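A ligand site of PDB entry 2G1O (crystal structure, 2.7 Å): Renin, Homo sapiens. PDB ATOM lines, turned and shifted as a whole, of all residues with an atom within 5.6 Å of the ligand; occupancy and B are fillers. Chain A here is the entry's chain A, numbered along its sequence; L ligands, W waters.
The side-chain carboxylate (OD1) of Asp 31 is in hydrogen-bond range of a nitrogen (N2) of the ligand, 2.5 Å away.
OD1 of Asp 219 lies within hydrogen-bond range of N4 of the ligand.
The side-chain hydroxyl of Thr 78 is in hydrogen-bond range of a nitrogen (N3) of the ligand (3.1 Å).
The side-chain hydroxyl of Ser 77 lies within hydrogen-bond range of a nitrogen (N3) of the ligand, at 3.2 Å.
Thr 11 touches the ligand (O to C15, 3.3 Å).
Gln 12 touches the ligand (NE2 to C22, 3.4 Å).
Tyr 13 touches the ligand (N to C16, 3.6 Å).
Val 29 touches the ligand (CG1 to C6, 3.6 Å).
CA of Gly 33 touches N4 of the ligand, at 3.5 Å.
Tyr 76 touches the ligand (CD2 to N2, 3.5 Å).
Pro 111 touches the ligand.
CE2 of Phe 112 touches C8 of the ligand, 3.8 Å away.
Leu 114 touches the ligand.
Ala 115 touches the ligand.
Phe 117 touches the ligand (CZ to C19, 3.6 Å).
CG2 of Val 120 touches C5 of the ligand, 3.8 Å away.
Thr 220 touches the ligand (O to C16, 3.4 Å).
Gly 221 touches the ligand.
Ser 223 touches the ligand (OG to C13, 3.5 Å).
19 residues have an atom within 4 Å of the ligand: Thr 11, Gln 12, Tyr 13, Val 29, Asp 31, Gly 33, Tyr 76, Ser 77, Thr 78, Pro 111, Phe 112, Leu 114, Ala 115, Phe 117, Val 120, Asp 219, Thr 220, Gly 221 and Ser 223.
The side-chain carboxylate of Asp 31 lies close to the backbone NH of Gly 221 (3.4 Å).
The side-chain carboxylate (OD1) of Asp 31 sits close to the backbone NH (N) of Ser 34 (3.3 Å).
The backbone NH of Gly 221 is in hydrogen-bond range of the side-chain carboxylate of Asp 219, 2.7 Å away.
The side-chain carboxylate (OD2) of Asp 219 sits at hydrogen-bond distance from the backbone NH (N) of Ala 222.
The side-chain hydroxyl (OG) of Ser 223 sits at hydrogen-bond distance from the backbone carbonyl oxygen (O) of Thr 11 (2.6 Å).
OE1 of Gln 12 sits at hydrogen-bond distance from N of Glu 116 (2.8 Å).
OH of Tyr 155 is in hydrogen-bond range of O of Thr 220 (2.7 Å).
The backbone carbonyl oxygen (O) of Ser 223 sits close to the backbone NH (N) of Ala 310 (3.3 Å).
Water W1 lies within hydrogen-bond range of a nitrogen (N1) of the ligand (3.1 Å) and the backbone NH (N) of Ser 77 (3.5 Å).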
ATOM      1  N   THR A  11      22.552 -32.300  20.243  1.00  0.00           N
ATOM      2  CA  THR A  11      22.405 -31.103  21.055  1.00  0.00           C
ATOM      3  C   THR A  11      22.409 -31.377  22.551  1.00  0.00           C
ATOM      4  O   THR A  11      22.346 -30.447  23.351  1.00  0.00           O
ATOM      5  CB  THR A  11      21.116 -30.372  20.735  1.00  0.00           C
ATOM      6  OG1 THR A  11      19.999 -31.236  20.988  1.00  0.00           O
ATOM      7  CG2 THR A  11      21.105 -29.930  19.282  1.00  0.00           C
ATOM      8  N   GLN A  12      22.490 -32.643  22.921  1.00  0.00           N
ATOM      9  CA  GLN A  12      22.491 -32.993  24.331  1.00  0.00           C
ATOM     10  C   GLN A  12      23.367 -34.212  24.576  1.00  0.00           C
ATOM     11  O   GLN A  12      23.143 -35.272  24.000  1.00  0.00           O
ATOM     12  CB  GLN A  12      21.065 -33.295  24.800  1.00  0.00           C
ATOM     13  CG  GLN A  12      20.185 -32.076  24.925  1.00  0.00           C
ATOM     14  CD  GLN A  12      18.789 -32.435  25.360  1.00  0.00           C
ATOM     15  OE1 GLN A  12      18.592 -33.238  26.284  1.00  0.00           O
ATOM     16  NE2 GLN A  12      17.794 -31.827  24.709  1.00  0.00           N
ATOM     17  N   TYR A  13      24.366 -34.051  25.447  1.00  0.00           N
ATOM     18  CA  TYR A  13      25.254 -35.152  25.777  1.00  0.00           C
ATOM     19  C   TYR A  13      25.191 -35.428  27.280  1.00  0.00           C
ATOM     20  O   TYR A  13      25.492 -34.560  28.094  1.00  0.00           O
ATOM     21  CB  TYR A  13      26.688 -34.847  25.356  1.00  0.00           C
ATOM     22  CG  TYR A  13      26.884 -34.798  23.863  1.00  0.00           C
ATOM     23  CD1 TYR A  13      26.568 -33.659  23.131  1.00  0.00           C
ATOM     24  CD2 TYR A  13      27.384 -35.900  23.171  1.00  0.00           C
ATOM     25  CE1 TYR A  13      26.728 -33.626  21.761  1.00  0.00           C
ATOM     26  CE2 TYR A  13      27.553 -35.866  21.796  1.00  0.00           C
ATOM     27  CZ  TYR A  13      27.224 -34.726  21.099  1.00  0.00           C
ATOM     28  OH  TYR A  13      27.383 -34.688  19.746  1.00  0.00           O
ATOM     29  N   VAL A  29      24.420 -33.953  32.411  1.00  0.00           N
ATOM     30  CA  VAL A  29      25.323 -33.339  31.436  1.00  0.00           C
ATOM     31  C   VAL A  29      26.576 -32.938  32.209  1.00  0.00           C
ATOM     32  O   VAL A  29      26.459 -32.325  33.268  1.00  0.00           O
ATOM     33  CB  VAL A  29      24.715 -32.078  30.823  1.00  0.00           C
ATOM     34  CG1 VAL A  29      25.727 -31.417  29.908  1.00  0.00           C
ATOM     35  CG2 VAL A  29      23.474 -32.409  30.059  1.00  0.00           C
ATOM     36  N   ASP A  31      29.174 -30.556  32.583  1.00  0.00           N
ATOM     37  CA  ASP A  31      29.328 -29.168  32.181  1.00  0.00           C
ATOM     38  C   ASP A  31      30.578 -28.431  32.666  1.00  0.00           C
ATOM     39  O   ASP A  31      30.721 -28.151  33.859  1.00  0.00           O
ATOM     40  CB  ASP A  31      28.076 -28.439  32.686  1.00  0.00           C
ATOM     41  CG  ASP A  31      28.015 -26.988  32.295  1.00  0.00           C
ATOM     42  OD1 ASP A  31      27.182 -26.284  32.896  1.00  0.00           O
ATOM     43  OD2 ASP A  31      28.772 -26.552  31.407  1.00  0.00           O
ATOM     44  N   GLY A  33      31.037 -25.615  31.930  1.00  0.00           N
ATOM     45  CA  GLY A  33      30.531 -24.253  31.998  1.00  0.00           C
ATOM     46  C   GLY A  33      29.893 -23.851  33.319  1.00  0.00           C
ATOM     47  O   GLY A  33      29.509 -22.704  33.489  1.00  0.00           O
ATOM     48  N   SER A  34      29.747 -24.793  34.248  1.00  0.00           N
ATOM     49  CA  SER A  34      29.188 -24.499  35.566  1.00  0.00           C
ATOM     50  C   SER A  34      30.019 -25.282  36.581  1.00  0.00           C
ATOM     51  O   SER A  34      30.933 -26.007  36.187  1.00  0.00           O
ATOM     52  CB  SER A  34      27.702 -24.886  35.632  1.00  0.00           C
ATOM     53  OG  SER A  34      27.485 -26.228  35.248  1.00  0.00           O
ATOM     54  N   TYR A  76      21.777 -20.362  34.233  1.00  0.00           N
ATOM     55  CA  TYR A  76      22.450 -20.662  32.975  1.00  0.00           C
ATOM     56  C   TYR A  76      21.973 -19.699  31.896  1.00  0.00           C
ATOM     57  O   TYR A  76      20.976 -19.009  32.057  1.00  0.00           O
ATOM     58  CB  TYR A  76      22.178 -22.120  32.551  1.00  0.00           C
ATOM     59  CG  TYR A  76      22.492 -23.139  33.615  1.00  0.00           C
ATOM     60  CD1 TYR A  76      21.490 -23.670  34.398  1.00  0.00           C
ATOM     61  CD2 TYR A  76      23.799 -23.572  33.836  1.00  0.00           C
ATOM     62  CE1 TYR A  76      21.768 -24.602  35.384  1.00  0.00           C
ATOM     63  CE2 TYR A  76      24.091 -24.507  34.824  1.00  0.00           C
ATOM     64  CZ  TYR A  76      23.071 -25.022  35.600  1.00  0.00           C
ATOM     65  OH  TYR A  76      23.321 -25.958  36.579  1.00  0.00           O
ATOM     66  N   SER A  77      22.694 -19.662  30.784  1.00  0.00           N
ATOM     67  CA  SER A  77      22.358 -18.769  29.691  1.00  0.00           C
ATOM     68  C   SER A  77      20.999 -19.069  29.078  1.00  0.00           C
ATOM     69  O   SER A  77      20.372 -18.206  28.480  1.00  0.00           O
ATOM     70  CB  SER A  77      23.421 -18.859  28.605  1.00  0.00           C
ATOM     71  OG  SER A  77      23.504 -20.166  28.077  1.00  0.00           O
ATOM     72  N   THR A  78      20.525 -20.298  29.257  1.00  0.00           N
ATOM     73  CA  THR A  78      19.258 -20.647  28.648  1.00  0.00           C
ATOM     74  C   THR A  78      18.183 -21.128  29.597  1.00  0.00           C
ATOM     75  O   THR A  78      17.190 -21.711  29.171  1.00  0.00           O
ATOM     76  CB  THR A  78      19.495 -21.712  27.571  1.00  0.00           C
ATOM     77  OG1 THR A  78      20.209 -22.806  28.146  1.00  0.00           O
ATOM     78  CG2 THR A  78      20.309 -21.138  26.443  1.00  0.00           C
ATOM     79  N   GLY A  79      18.367 -20.865  30.884  1.00  0.00           N
ATOM     80  CA  GLY A  79      17.379 -21.295  31.861  1.00  0.00           C
ATOM     81  C   GLY A  79      17.911 -21.271  33.276  1.00  0.00           C
ATOM     82  O   GLY A  79      19.110 -21.166  33.507  1.00  0.00           O
ATOM     83  N   PRO A 111      12.954 -24.251  29.719  1.00  0.00           N
ATOM     84  CA  PRO A 111      13.161 -25.286  28.690  1.00  0.00           C
ATOM     85  C   PRO A 111      13.271 -26.728  29.154  1.00  0.00           C
ATOM     86  O   PRO A 111      13.328 -27.638  28.329  1.00  0.00           O
ATOM     87  CB  PRO A 111      14.469 -24.842  28.081  1.00  0.00           C
ATOM     88  CG  PRO A 111      15.253 -24.492  29.336  1.00  0.00           C
ATOM     89  CD  PRO A 111      14.243 -23.727  30.183  1.00  0.00           C
ATOM     90  N   PHE A 112      13.302 -26.972  30.461  1.00  0.00           N
ATOM     91  CA  PHE A 112      13.511 -28.331  30.920  1.00  0.00           C
ATOM     92  C   PHE A 112      12.629 -29.480  30.469  1.00  0.00           C
ATOM     93  O   PHE A 112      13.014 -30.630  30.584  1.00  0.00           O
ATOM     94  CB  PHE A 112      13.703 -28.322  32.439  1.00  0.00           C
ATOM     95  CG  PHE A 112      14.934 -27.555  32.846  1.00  0.00           C
ATOM     96  CD1 PHE A 112      14.840 -26.230  33.233  1.00  0.00           C
ATOM     97  CD2 PHE A 112      16.186 -28.116  32.720  1.00  0.00           C
ATOM     98  CE1 PHE A 112      15.975 -25.487  33.475  1.00  0.00           C
ATOM     99  CE2 PHE A 112      17.319 -27.382  32.959  1.00  0.00           C
ATOM    100  CZ  PHE A 112      17.219 -26.063  33.335  1.00  0.00           C
ATOM    101  N   MET A 113      11.444 -29.181  29.929  1.00  0.00           N
ATOM    102  CA  MET A 113      10.570 -30.233  29.412  1.00  0.00           C
ATOM    103  C   MET A 113      11.214 -30.776  28.155  1.00  0.00           C
ATOM    104  O   MET A 113      10.882 -31.881  27.699  1.00  0.00           O
ATOM    105  CB  MET A 113       9.188 -29.698  29.055  1.00  0.00           C
ATOM    106  CG  MET A 113       8.147 -29.808  30.151  1.00  0.00           C
ATOM    107  SD  MET A 113       7.975 -31.492  30.797  1.00  0.00           S
ATOM    108  CE  MET A 113       7.790 -32.409  29.328  1.00  0.00           C
ATOM    109  N   LEU A 114      12.144 -30.011  27.596  1.00  0.00           N
ATOM    110  CA  LEU A 114      12.845 -30.419  26.386  1.00  0.00           C
ATOM    111  C   LEU A 114      14.137 -31.178  26.690  1.00  0.00           C
ATOM    112  O   LEU A 114      14.784 -31.702  25.780  1.00  0.00           O
ATOM    113  CB  LEU A 114      13.171 -29.197  25.523  1.00  0.00           C
ATOM    114  CG  LEU A 114      11.974 -28.379  25.007  1.00  0.00           C
ATOM    115  CD1 LEU A 114      12.512 -27.250  24.161  1.00  0.00           C
ATOM    116  CD2 LEU A 114      11.038 -29.251  24.185  1.00  0.00           C
ATOM    117  N   ALA A 115      14.506 -31.229  27.964  1.00  0.00           N
ATOM    118  CA  ALA A 115      15.715 -31.919  28.386  1.00  0.00           C
ATOM    119  C   ALA A 115      15.536 -33.423  28.451  1.00  0.00           C
ATOM    120  O   ALA A 115      14.532 -33.905  28.969  1.00  0.00           O
ATOM    121  CB  ALA A 115      16.143 -31.419  29.739  1.00  0.00           C
ATOM    122  N   GLU A 116      16.515 -34.143  27.921  1.00  0.00           N
ATOM    123  CA  GLU A 116      16.502 -35.602  27.968  1.00  0.00           C
ATOM    124  C   GLU A 116      17.214 -35.997  29.245  1.00  0.00           C
ATOM    125  O   GLU A 116      16.973 -37.063  29.805  1.00  0.00           O
ATOM    126  CB  GLU A 116      17.234 -36.182  26.748  1.00  0.00           C
ATOM    127  CG  GLU A 116      16.331 -36.461  25.559  1.00  0.00           C
ATOM    128  CD  GLU A 116      15.589 -37.781  25.690  1.00  0.00           C
ATOM    129  OE1 GLU A 116      16.259 -38.835  25.738  1.00  0.00           O
ATOM    130  OE2 GLU A 116      14.346 -37.760  25.731  1.00  0.00           O
ATOM    131  N   PHE A 117      18.098 -35.135  29.721  1.00  0.00           N
ATOM    132  CA  PHE A 117      18.832 -35.396  30.939  1.00  0.00           C
ATOM    133  C   PHE A 117      17.998 -34.973  32.133  1.00  0.00           C
ATOM    134  O   PHE A 117      17.014 -34.239  31.977  1.00  0.00           O
ATOM    135  CB  PHE A 117      20.155 -34.622  30.944  1.00  0.00           C
ATOM    136  CG  PHE A 117      20.000 -33.153  30.668  1.00  0.00           C
ATOM    137  CD1 PHE A 117      19.875 -32.684  29.373  1.00  0.00           C
ATOM    138  CD2 PHE A 117      19.994 -32.230  31.712  1.00  0.00           C
ATOM    139  CE1 PHE A 117      19.747 -31.314  29.124  1.00  0.00           C
ATOM    140  CE2 PHE A 117      19.869 -30.873  31.467  1.00  0.00           C
ATOM    141  CZ  PHE A 117      19.752 -30.413  30.164  1.00  0.00           C
ATOM    142  N   VAL A 120      22.561 -31.771  36.190  1.00  0.00           N
ATOM    143  CA  VAL A 120      23.887 -31.347  35.783  1.00  0.00           C
ATOM    144  C   VAL A 120      25.023 -31.593  36.775  1.00  0.00           C
ATOM    145  O   VAL A 120      24.857 -31.486  37.990  1.00  0.00           O
ATOM    146  CB  VAL A 120      23.882 -29.843  35.429  1.00  0.00           C
ATOM    147  CG1 VAL A 120      25.230 -29.443  34.838  1.00  0.00           C
ATOM    148  CG2 VAL A 120      22.725 -29.557  34.483  1.00  0.00           C
ATOM    149  N   TYR A 155      32.841 -36.060  22.048  1.00  0.00           N
ATOM    150  CA  TYR A 155      31.436 -35.986  21.640  1.00  0.00           C
ATOM    151  C   TYR A 155      31.374 -36.489  20.221  1.00  0.00           C
ATOM    152  O   TYR A 155      31.881 -35.835  19.309  1.00  0.00           O
ATOM    153  CB  TYR A 155      30.918 -34.547  21.647  1.00  0.00           C
ATOM    154  CG  TYR A 155      30.502 -34.033  23.005  1.00  0.00           C
ATOM    155  CD1 TYR A 155      30.216 -32.685  23.199  1.00  0.00           C
ATOM    156  CD2 TYR A 155      30.424 -34.882  24.098  1.00  0.00           C
ATOM    157  CE1 TYR A 155      29.870 -32.195  24.443  1.00  0.00           C
ATOM    158  CE2 TYR A 155      30.068 -34.402  25.345  1.00  0.00           C
ATOM    159  CZ  TYR A 155      29.794 -33.055  25.504  1.00  0.00           C
ATOM    160  OH  TYR A 155      29.450 -32.556  26.751  1.00  0.00           O
ATOM    161  N   ASP A 219      32.902 -24.603  26.627  1.00  0.00           N
ATOM    162  CA  ASP A 219      31.770 -25.155  27.375  1.00  0.00           C
ATOM    163  C   ASP A 219      31.217 -26.500  26.941  1.00  0.00           C
ATOM    164  O   ASP A 219      30.506 -26.590  25.950  1.00  0.00           O
ATOM    165  CB  ASP A 219      30.664 -24.098  27.363  1.00  0.00           C
ATOM    166  CG  ASP A 219      29.587 -24.374  28.369  1.00  0.00           C
ATOM    167  OD1 ASP A 219      28.772 -23.461  28.608  1.00  0.00           O
ATOM    168  OD2 ASP A 219      29.549 -25.490  28.919  1.00  0.00           O
ATOM    169  N   THR A 220      31.526 -27.558  27.689  1.00  0.00           N
ATOM    170  CA  THR A 220      31.020 -28.890  27.345  1.00  0.00           C
ATOM    171  C   THR A 220      29.511 -29.011  27.550  1.00  0.00           C
ATOM    172  O   THR A 220      28.874 -29.916  27.023  1.00  0.00           O
ATOM    173  CB  THR A 220      31.684 -30.002  28.183  1.00  0.00           C
ATOM    174  OG1 THR A 220      31.457 -29.744  29.577  1.00  0.00           O
ATOM    175  CG2 THR A 220      33.162 -30.091  27.890  1.00  0.00           C
ATOM    176  N   GLY A 221      28.956 -28.105  28.335  1.00  0.00           N
ATOM    177  CA  GLY A 221      27.536 -28.137  28.610  1.00  0.00           C
ATOM    178  C   GLY A 221      26.691 -27.287  27.688  1.00  0.00           C
ATOM    179  O   GLY A 221      25.491 -27.149  27.897  1.00  0.00           O
ATOM    180  N   ALA A 222      27.313 -26.726  26.651  1.00  0.00           N
ATOM    181  CA  ALA A 222      26.594 -25.901  25.681  1.00  0.00           C
ATOM    182  C   ALA A 222      26.476 -26.635  24.367  1.00  0.00           C
ATOM    183  O   ALA A 222      27.421 -27.265  23.903  1.00  0.00           O
ATOM    184  CB  ALA A 222      27.329 -24.590  25.486  1.00  0.00           C
ATOM    185  N   SER A 223      25.300 -26.555  23.746  1.00  0.00           N
ATOM    186  CA  SER A 223      25.062 -27.242  22.473  1.00  0.00           C
ATOM    187  C   SER A 223      25.857 -26.691  21.296  1.00  0.00           C
ATOM    188  O   SER A 223      26.529 -27.431  20.596  1.00  0.00           O
ATOM    189  CB  SER A 223      23.591 -27.204  22.108  1.00  0.00           C
ATOM    190  OG  SER A 223      22.812 -27.919  23.041  1.00  0.00           O
ATOM    191  N   ALA A 310      29.355 -28.034  22.096  1.00  0.00           N
ATOM    192  CA  ALA A 310      29.314 -29.309  21.408  1.00  0.00           C
ATOM    193  C   ALA A 310      29.681 -29.246  19.918  1.00  0.00           C
ATOM    194  O   ALA A 310      30.359 -30.138  19.406  1.00  0.00           O
ATOM    195  CB  ALA A 310      27.943 -29.944  21.580  1.00  0.00           C
HETATM  196  C1  LIG L   1      23.946 -24.008  29.601  1.00  0.00           C
HETATM  197  N1  LIG L   1      25.202 -23.556  29.793  1.00  0.00           N
HETATM  198  C2  LIG L   1      25.959 -24.242  30.656  1.00  0.00           C
HETATM  199  N2  LIG L   1      25.544 -25.322  31.333  1.00  0.00           N
HETATM  200  C3  LIG L   1      24.287 -25.800  31.155  1.00  0.00           C
HETATM  201  C4  LIG L   1      23.407 -25.143  30.249  1.00  0.00           C
HETATM  202  N3  LIG L   1      23.211 -23.297  28.720  1.00  0.00           N
HETATM  203  N4  LIG L   1      27.224 -23.833  30.875  1.00  0.00           N
HETATM  204  C5  LIG L   1      23.907 -27.030  31.974  1.00  0.00           C
HETATM  205  C6  LIG L   1      24.359 -28.339  31.313  1.00  0.00           C
HETATM  206  C7  LIG L   1      20.841 -25.400  30.736  1.00  0.00           C
HETATM  207  C8  LIG L   1      19.586 -25.976  30.316  1.00  0.00           C
HETATM  208  C9  LIG L   1      19.553 -26.761  29.140  1.00  0.00           C
HETATM  209  C10 LIG L   1      20.708 -26.958  28.411  1.00  0.00           C
HETATM  210  C11 LIG L   1      21.930 -26.413  28.815  1.00  0.00           C
HETATM  211  C12 LIG L   1      22.024 -25.632  29.972  1.00  0.00           C
HETATM  212  N5  LIG L   1      20.468 -27.745  27.304  1.00  0.00           N
HETATM  213  C13 LIG L   1      21.509 -28.138  26.330  1.00  0.00           C
HETATM  214  C14 LIG L   1      22.322 -29.367  26.786  1.00  0.00           C
HETATM  215  C15 LIG L   1      23.713 -29.434  26.133  1.00  0.00           C
HETATM  216  O1  LIG L   1      24.402 -30.591  26.592  1.00  0.00           O
HETATM  217  C16 LIG L   1      25.698 -30.780  26.055  1.00  0.00           C
HETATM  218  C17 LIG L   1      18.402 -28.867  26.357  1.00  0.00           C
HETATM  219  C18 LIG L   1      19.130 -28.075  27.291  1.00  0.00           C
HETATM  220  C19 LIG L   1      18.500 -27.498  28.411  1.00  0.00           C
HETATM  221  C20 LIG L   1      17.120 -27.681  28.639  1.00  0.00           C
HETATM  222  C21 LIG L   1      16.363 -28.471  27.714  1.00  0.00           C
HETATM  223  C22 LIG L   1      17.006 -29.066  26.577  1.00  0.00           C
HETATM  224  O   HOH W   1      25.650 -21.223  31.778  1.00  0.00           O
